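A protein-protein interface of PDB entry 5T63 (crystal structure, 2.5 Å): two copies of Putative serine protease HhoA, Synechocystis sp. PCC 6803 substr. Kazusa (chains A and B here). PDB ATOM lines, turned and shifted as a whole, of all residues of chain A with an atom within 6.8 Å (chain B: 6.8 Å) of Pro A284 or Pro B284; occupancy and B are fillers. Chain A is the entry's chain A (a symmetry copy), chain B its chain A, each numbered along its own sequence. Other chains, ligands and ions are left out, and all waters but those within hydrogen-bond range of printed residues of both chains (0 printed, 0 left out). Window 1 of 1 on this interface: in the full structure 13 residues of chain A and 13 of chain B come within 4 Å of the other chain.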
ATOM      1  N   ASN A 277      -9.691  -4.169  -0.975  1.00  0.00           N
ATOM      2  CA  ASN A 277     -10.887  -4.888  -0.579  1.00  0.00           C
ATOM      3  C   ASN A 277     -12.140  -4.278  -1.176  1.00  0.00           C
ATOM      4  O   ASN A 277     -13.059  -5.004  -1.569  1.00  0.00           O
ATOM      5  CB  ASN A 277     -10.992  -4.892   0.944  1.00  0.00           C
ATOM      6  CG  ASN A 277     -12.326  -5.428   1.425  1.00  0.00           C
ATOM      7  OD1 ASN A 277     -12.438  -6.590   1.790  1.00  0.00           O
ATOM      8  ND2 ASN A 277     -13.338  -4.576   1.437  1.00  0.00           N
ATOM      9  N   ASN A 280     -13.344  -5.062  -4.878  1.00  0.00           N
ATOM     10  CA  ASN A 280     -13.875  -6.371  -5.235  1.00  0.00           C
ATOM     11  C   ASN A 280     -15.388  -6.403  -5.024  1.00  0.00           C
ATOM     12  O   ASN A 280     -15.846  -6.313  -3.873  1.00  0.00           O
ATOM     13  CB  ASN A 280     -13.191  -7.456  -4.422  1.00  0.00           C
ATOM     14  CG  ASN A 280     -13.802  -8.851  -4.625  1.00  0.00           C
ATOM     15  OD1 ASN A 280     -14.890  -9.034  -5.181  1.00  0.00           O
ATOM     16  ND2 ASN A 280     -13.091  -9.846  -4.141  1.00  0.00           N
ATOM     17  N   PRO A 281     -16.188  -6.597  -6.079  1.00  0.00           N
ATOM     18  CA  PRO A 281     -17.644  -6.586  -5.901  1.00  0.00           C
ATOM     19  C   PRO A 281     -18.109  -7.590  -4.885  1.00  0.00           C
ATOM     20  O   PRO A 281     -19.201  -7.407  -4.317  1.00  0.00           O
ATOM     21  CB  PRO A 281     -18.184  -6.908  -7.302  1.00  0.00           C
ATOM     22  CG  PRO A 281     -17.059  -6.640  -8.238  1.00  0.00           C
ATOM     23  CD  PRO A 281     -15.798  -6.908  -7.463  1.00  0.00           C
ATOM     24  N   ASN A 282     -17.296  -8.609  -4.582  1.00  0.00           N
ATOM     25  CA  ASN A 282     -17.749  -9.709  -3.733  1.00  0.00           C
ATOM     26  C   ASN A 282     -17.115  -9.718  -2.348  1.00  0.00           C
ATOM     27  O   ASN A 282     -17.328 -10.669  -1.596  1.00  0.00           O
ATOM     28  CB  ASN A 282     -17.492 -11.051  -4.417  1.00  0.00           C
ATOM     29  CG  ASN A 282     -18.485 -11.335  -5.505  1.00  0.00           C
ATOM     30  OD1 ASN A 282     -19.688 -11.155  -5.314  1.00  0.00           O
ATOM     31  ND2 ASN A 282     -18.000 -11.784  -6.649  1.00  0.00           N
ATOM     32  N   SER A 283     -16.348  -8.703  -1.977  1.00  0.00           N
ATOM     33  CA  SER A 283     -15.933  -8.651  -0.585  1.00  0.00           C
ATOM     34  C   SER A 283     -17.165  -8.531   0.328  1.00  0.00           C
ATOM     35  O   SER A 283     -18.187  -7.938  -0.048  1.00  0.00           O
ATOM     36  CB  SER A 283     -14.952  -7.497  -0.351  1.00  0.00           C
ATOM     37  OG  SER A 283     -15.565  -6.248  -0.561  1.00  0.00           O
ATOM     38  N   PRO A 284     -17.106  -9.108   1.533  1.00  0.00           N
ATOM     39  CA  PRO A 284     -18.317  -9.141   2.365  1.00  0.00           C
ATOM     40  C   PRO A 284     -18.769  -7.769   2.860  1.00  0.00           C
ATOM     41  O   PRO A 284     -19.980  -7.484   2.881  1.00  0.00           O
ATOM     42  CB  PRO A 284     -17.916 -10.068   3.516  1.00  0.00           C
ATOM     43  CG  PRO A 284     -16.461  -9.977   3.597  1.00  0.00           C
ATOM     44  CD  PRO A 284     -15.942  -9.730   2.199  1.00  0.00           C
ATOM     45  N   PHE A 285     -17.842  -6.903   3.257  1.00  0.00           N
ATOM     46  CA  PHE A 285     -18.213  -5.568   3.698  1.00  0.00           C
ATOM     47  C   PHE A 285     -17.283  -4.524   3.107  1.00  0.00           C
ATOM     48  O   PHE A 285     -16.114  -4.791   2.816  1.00  0.00           O
ATOM     49  CB  PHE A 285     -18.213  -5.457   5.226  1.00  0.00           C
ATOM     50  CG  PHE A 285     -17.075  -6.179   5.901  1.00  0.00           C
ATOM     51  CD1 PHE A 285     -17.211  -7.515   6.286  1.00  0.00           C
ATOM     52  CD2 PHE A 285     -15.872  -5.524   6.149  1.00  0.00           C
ATOM     53  CE1 PHE A 285     -16.172  -8.189   6.932  1.00  0.00           C
ATOM     54  CE2 PHE A 285     -14.836  -6.186   6.787  1.00  0.00           C
ATOM     55  CZ  PHE A 285     -14.978  -7.528   7.190  1.00  0.00           C
ATOM     56  N   ILE A 286     -17.836  -3.328   2.922  1.00  0.00           N
ATOM     57  CA  ILE A 286     -17.044  -2.151   2.595  1.00  0.00           C
ATOM     58  C   ILE A 286     -16.248  -1.717   3.818  1.00  0.00           C
ATOM     59  O   ILE A 286     -16.805  -1.597   4.920  1.00  0.00           O
ATOM     60  CB  ILE A 286     -17.965  -1.023   2.119  1.00  0.00           C
ATOM     61  CG1 ILE A 286     -18.474  -1.315   0.713  1.00  0.00           C
ATOM     62  CG2 ILE A 286     -17.241   0.327   2.225  1.00  0.00           C
ATOM     63  CD1 ILE A 286     -19.652  -0.419   0.323  1.00  0.00           C
ATOM     64  N   ARG A 310     -19.198  -6.174  16.105  1.00  0.00           N
ATOM     65  CA  ARG A 310     -19.621  -6.986  14.982  1.00  0.00           C
ATOM     66  C   ARG A 310     -18.470  -7.197  14.023  1.00  0.00           C
ATOM     67  O   ARG A 310     -17.671  -6.282  13.794  1.00  0.00           O
ATOM     68  CB  ARG A 310     -20.754  -6.322  14.200  1.00  0.00           C
ATOM     69  CG  ARG A 310     -22.026  -6.004  14.957  1.00  0.00           C
ATOM     70  CD  ARG A 310     -23.051  -5.444  13.940  1.00  0.00           C
ATOM     71  NE  ARG A 310     -22.923  -6.145  12.659  1.00  0.00           N
ATOM     72  CZ  ARG A 310     -23.444  -7.345  12.411  1.00  0.00           C
ATOM     73  NH1 ARG A 310     -24.159  -7.968  13.370  1.00  0.00           N
ATOM     74  NH2 ARG A 310     -23.230  -7.921  11.219  1.00  0.00           N
ATOM     75  N   ARG A 311     -18.423  -8.384  13.426  1.00  0.00           N
ATOM     76  CA  ARG A 311     -17.606  -8.597  12.246  1.00  0.00           C
ATOM     77  C   ARG A 311     -17.729  -7.413  11.301  1.00  0.00           C
ATOM     78  O   ARG A 311     -18.833  -6.996  10.950  1.00  0.00           O
ATOM     79  CB  ARG A 311     -18.061  -9.856  11.536  1.00  0.00           C
ATOM     80  CG  ARG A 311     -17.366 -10.067  10.220  1.00  0.00           C
ATOM     81  CD  ARG A 311     -17.943 -11.295   9.552  1.00  0.00           C
ATOM     82  NE  ARG A 311     -17.186 -11.642   8.362  1.00  0.00           N
ATOM     83  CZ  ARG A 311     -17.576 -12.550   7.486  1.00  0.00           C
ATOM     84  NH1 ARG A 311     -18.724 -13.185   7.682  1.00  0.00           N
ATOM     85  NH2 ARG A 311     -16.827 -12.805   6.427  1.00  0.00           N
ATOM     86  N   GLY A 312     -16.590  -6.869  10.896  1.00  0.00           N
ATOM     87  CA  GLY A 312     -16.535  -5.731  10.022  1.00  0.00           C
ATOM     88  C   GLY A 312     -16.174  -4.427  10.709  1.00  0.00           C
ATOM     89  O   GLY A 312     -15.759  -3.497  10.041  1.00  0.00           O
ATOM     90  N   ASN B 277     -30.673 -12.263  10.386  1.00  0.00           N
ATOM     91  CA  ASN B 277     -29.310 -12.054   9.935  1.00  0.00           C
ATOM     92  C   ASN B 277     -28.615 -10.957  10.718  1.00  0.00           C
ATOM     93  O   ASN B 277     -27.421 -11.069  11.019  1.00  0.00           O
ATOM     94  CB  ASN B 277     -29.319 -11.699   8.450  1.00  0.00           C
ATOM     95  CG  ASN B 277     -27.958 -11.248   7.959  1.00  0.00           C
ATOM     96  OD1 ASN B 277     -27.211 -12.028   7.384  1.00  0.00           O
ATOM     97  ND2 ASN B 277     -27.637  -9.984   8.178  1.00  0.00           N
ATOM     98  N   ASN B 280     -26.947 -11.593  14.265  1.00  0.00           N
ATOM     99  CA  ASN B 280     -25.730 -12.383  14.394  1.00  0.00           C
ATOM    100  C   ASN B 280     -24.500 -11.483  14.277  1.00  0.00           C
ATOM    101  O   ASN B 280     -24.256 -10.921  13.197  1.00  0.00           O
ATOM    102  CB  ASN B 280     -25.701 -13.480  13.343  1.00  0.00           C
ATOM    103  CG  ASN B 280     -24.378 -14.261  13.309  1.00  0.00           C
ATOM    104  OD1 ASN B 280     -23.356 -13.878  13.887  1.00  0.00           O
ATOM    105  ND2 ASN B 280     -24.403 -15.366  12.596  1.00  0.00           N
ATOM    106  N   PRO B 281     -23.673 -11.374  15.322  1.00  0.00           N
ATOM    107  CA  PRO B 281     -22.512 -10.480  15.243  1.00  0.00           C
ATOM    108  C   PRO B 281     -21.614 -10.801  14.084  1.00  0.00           C
ATOM    109  O   PRO B 281     -20.874  -9.908  13.633  1.00  0.00           O
ATOM    110  CB  PRO B 281     -21.798 -10.691  16.586  1.00  0.00           C
ATOM    111  CG  PRO B 281     -22.805 -11.320  17.483  1.00  0.00           C
ATOM    112  CD  PRO B 281     -23.718 -12.117  16.592  1.00  0.00           C
ATOM    113  N   ASN B 282     -21.696 -12.021  13.536  1.00  0.00           N
ATOM    114  CA  ASN B 282     -20.741 -12.457  12.520  1.00  0.00           C
ATOM    115  C   ASN B 282     -21.336 -12.565  11.122  1.00  0.00           C
ATOM    116  O   ASN B 282     -20.656 -13.043  10.214  1.00  0.00           O
ATOM    117  CB  ASN B 282     -20.121 -13.798  12.912  1.00  0.00           C
ATOM    118  CG  ASN B 282     -19.082 -13.653  13.984  1.00  0.00           C
ATOM    119  OD1 ASN B 282     -18.227 -12.771  13.909  1.00  0.00           O
ATOM    120  ND2 ASN B 282     -19.139 -14.513  14.986  1.00  0.00           N
ATOM    121  N   SER B 283     -22.574 -12.141  10.908  1.00  0.00           N
ATOM    122  CA  SER B 283     -23.028 -12.071   9.529  1.00  0.00           C
ATOM    123  C   SER B 283     -22.159 -11.079   8.737  1.00  0.00           C
ATOM    124  O   SER B 283     -21.656 -10.088   9.286  1.00  0.00           O
ATOM    125  CB  SER B 283     -24.511 -11.690   9.462  1.00  0.00           C
ATOM    126  OG  SER B 283     -24.731 -10.388   9.950  1.00  0.00           O
ATOM    127  N   PRO B 284     -21.947 -11.333   7.442  1.00  0.00           N
ATOM    128  CA  PRO B 284     -21.001 -10.490   6.698  1.00  0.00           C
ATOM    129  C   PRO B 284     -21.469  -9.049   6.510  1.00  0.00           C
ATOM    130  O   PRO B 284     -20.657  -8.112   6.621  1.00  0.00           O
ATOM    131  CB  PRO B 284     -20.857 -11.231   5.365  1.00  0.00           C
ATOM    132  CG  PRO B 284     -22.092 -11.993   5.211  1.00  0.00           C
ATOM    133  CD  PRO B 284     -22.567 -12.375   6.595  1.00  0.00           C
ATOM    134  N   PHE B 285     -22.750  -8.831   6.230  1.00  0.00           N
ATOM    135  CA  PHE B 285     -23.258  -7.477   6.082  1.00  0.00           C
ATOM    136  C   PHE B 285     -24.583  -7.313   6.805  1.00  0.00           C
ATOM    137  O   PHE B 285     -25.354  -8.262   6.964  1.00  0.00           O
ATOM    138  CB  PHE B 285     -23.420  -7.091   4.609  1.00  0.00           C
ATOM    139  CG  PHE B 285     -23.961  -8.194   3.735  1.00  0.00           C
ATOM    140  CD1 PHE B 285     -23.096  -9.092   3.107  1.00  0.00           C
ATOM    141  CD2 PHE B 285     -25.333  -8.332   3.543  1.00  0.00           C
ATOM    142  CE1 PHE B 285     -23.583 -10.104   2.276  1.00  0.00           C
ATOM    143  CE2 PHE B 285     -25.825  -9.335   2.723  1.00  0.00           C
ATOM    144  CZ  PHE B 285     -24.951 -10.231   2.077  1.00  0.00           C
ATOM    145  N   ILE B 286     -24.822  -6.083   7.255  1.00  0.00           N
ATOM    146  CA  ILE B 286     -26.130  -5.683   7.753  1.00  0.00           C
ATOM    147  C   ILE B 286     -27.105  -5.567   6.590  1.00  0.00           C
ATOM    148  O   ILE B 286     -26.795  -4.933   5.571  1.00  0.00           O
ATOM    149  CB  ILE B 286     -26.013  -4.349   8.497  1.00  0.00           C
ATOM    150  CG1 ILE B 286     -25.341  -4.554   9.849  1.00  0.00           C
ATOM    151  CG2 ILE B 286     -27.394  -3.687   8.610  1.00  0.00           C
ATOM    152  CD1 ILE B 286     -24.887  -3.236  10.480  1.00  0.00           C
ATOM    153  N   ARG B 310     -22.896  -4.962  -6.116  1.00  0.00           N
ATOM    154  CA  ARG B 310     -22.008  -5.573  -5.148  1.00  0.00           C
ATOM    155  C   ARG B 310     -22.755  -6.599  -4.324  1.00  0.00           C
ATOM    156  O   ARG B 310     -23.921  -6.389  -3.972  1.00  0.00           O
ATOM    157  CB  ARG B 310     -21.429  -4.541  -4.181  1.00  0.00           C
ATOM    158  CG  ARG B 310     -20.634  -3.399  -4.780  1.00  0.00           C
ATOM    159  CD  ARG B 310     -20.068  -2.557  -3.610  1.00  0.00           C
ATOM    160  NE  ARG B 310     -19.680  -3.434  -2.501  1.00  0.00           N
ATOM    161  CZ  ARG B 310     -18.541  -4.123  -2.459  1.00  0.00           C
ATOM    162  NH1 ARG B 310     -17.660  -4.009  -3.473  1.00  0.00           N
ATOM    163  NH2 ARG B 310     -18.303  -4.934  -1.418  1.00  0.00           N
ATOM    164  N   ARG B 311     -22.062  -7.678  -3.974  1.00  0.00           N
ATOM    165  CA  ARG B 311     -22.523  -8.553  -2.913  1.00  0.00           C
ATOM    166  C   ARG B 311     -23.055  -7.732  -1.749  1.00  0.00           C
ATOM    167  O   ARG B 311     -22.384  -6.827  -1.254  1.00  0.00           O
ATOM    168  CB  ARG B 311     -21.374  -9.417  -2.434  1.00  0.00           C
ATOM    169  CG  ARG B 311     -21.730 -10.246  -1.231  1.00  0.00           C
ATOM    170  CD  ARG B 311     -20.502 -11.006  -0.780  1.00  0.00           C
ATOM    171  NE  ARG B 311     -20.837 -11.953   0.270  1.00  0.00           N
ATOM    172  CZ  ARG B 311     -19.934 -12.611   0.974  1.00  0.00           C
ATOM    173  NH1 ARG B 311     -18.647 -12.403   0.732  1.00  0.00           N
ATOM    174  NH2 ARG B 311     -20.324 -13.456   1.914  1.00  0.00           N
ATOM    175  N   GLY B 312     -24.269  -8.048  -1.319  1.00  0.00           N
ATOM    176  CA  GLY B 312     -24.923  -7.354  -0.246  1.00  0.00           C
ATOM    177  C   GLY B 312     -26.020  -6.404  -0.687  1.00  0.00           C
ATOM    178  O   GLY B 312     -26.857  -6.044   0.122  1.00  0.00           O
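The backbone carbonyl oxygen (O) of Asn B280 is in hydrogen-bond range of the guanidinium group (NH1) of Arg A310 (3.0 Å).
The backbone carbonyl oxygen (O) of Pro B281 lies within hydrogen-bond range of the backbone NH (N) of Arg A311 (2.9 Å).
O of Asn B282 lies within hydrogen-bond range of NH1 of Arg A311 (3.2 Å).
The side-chain hydroxyl (OG) of Ser B283 sits at hydrogen-bond distance from the guanidinium group (NH2) of Arg A310, at 3.2 Å.
The guanidinium group (NH1) of Arg B310 sits at hydrogen-bond distance from the backbone carbonyl oxygen (O) of Asn A280 (3.0 Å).
The guanidinium group (NH2) of Arg B310 lies within hydrogen-bond range of the side-chain hydroxyl (OG) of Ser A283.
O of Pro A281 lies within hydrogen-bond range of N of Arg B311 (2.9 Å).
The backbone carbonyl oxygen (O) of Asn A282 is in hydrogen-bond range of the guanidinium group (NH1) of Arg B311, 3.2 Å away.
Of the printed residues of chain B, Asn A280 touches Arg B310 (3.0 Å).
Of chain B, only Pro B284, Phe B285 and Arg B311 come within 4 Å of Pro A284.
Printed residues of chain B within 4 Å of Phe A285: Pro B284.
Printed residues of chain A within 4 Å of Pro B281: Arg A310 and Arg A311.
Pro B284 touches just these residues of chain A: Pro A284 (3.7 Å), Phe A285 (3.5 Å) and Arg A311 (3.7 Å).
Of the printed residues of chain A, Phe B285 touches Pro A284.
The nearest residue of chain A that does not touch Pro B284 is Arg A310 (5.2 Å).
Asn A280 touches Arg B310, and with the chains exchanged Arg A310 touches Asn B280.
Ser A283 touches Arg B311, and with the chains exchanged Arg A311 touches Ser B283.
Pro A284 touches its own counterpart, Pro B284.
Pro A284 touches Phe B285, and with the chains exchanged Phe A285 touches Pro B284.
Of the 17 pairs that touch across the chains among the printed residues, 17 have their exchanged pair printed and touching as well.
Of the 11 printed residues of chain B, 8 touch a printed residue of chain A.
Hydrophobic or aromatic side chains of chain B that line the printed part of chain A: Pro B284 and Phe B285.
Among the printed residues, pairs that only touch across the chains: Arg A310 with Pro B281, Pro A281 with Arg B310, Phe A285 with Pro B284, Pro A284 with Phe B285, Arg A311 with Pro B284, Pro A284 with Arg B311, Pro A284 with Pro B284, Ser A283 with Arg B311 and Arg A311 with Ser B283.
O of Asn B277 lies within hydrogen-bond range of OG of Ser B283.
ND2 of Asn B277 is in hydrogen-bond range of O of Phe B285 (3.1 Å).
OG of Ser B283 sits at hydrogen-bond distance from O of Asn B280, at 3.3 Å.
The side-chain amide nitrogen (ND2) of Asn A277 is in hydrogen-bond range of the backbone carbonyl oxygen (O) of Phe A285 (3.1 Å).
The side-chain amide oxygen (OD1) of Asn A280 lies within hydrogen-bond range of the backbone NH (N) of Asn A282 (2.5 Å).
The backbone carbonyl oxygen (O) of Asn A280 is in hydrogen-bond range of the side-chain hydroxyl (OG) of Ser A283, 3.3 Å away.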
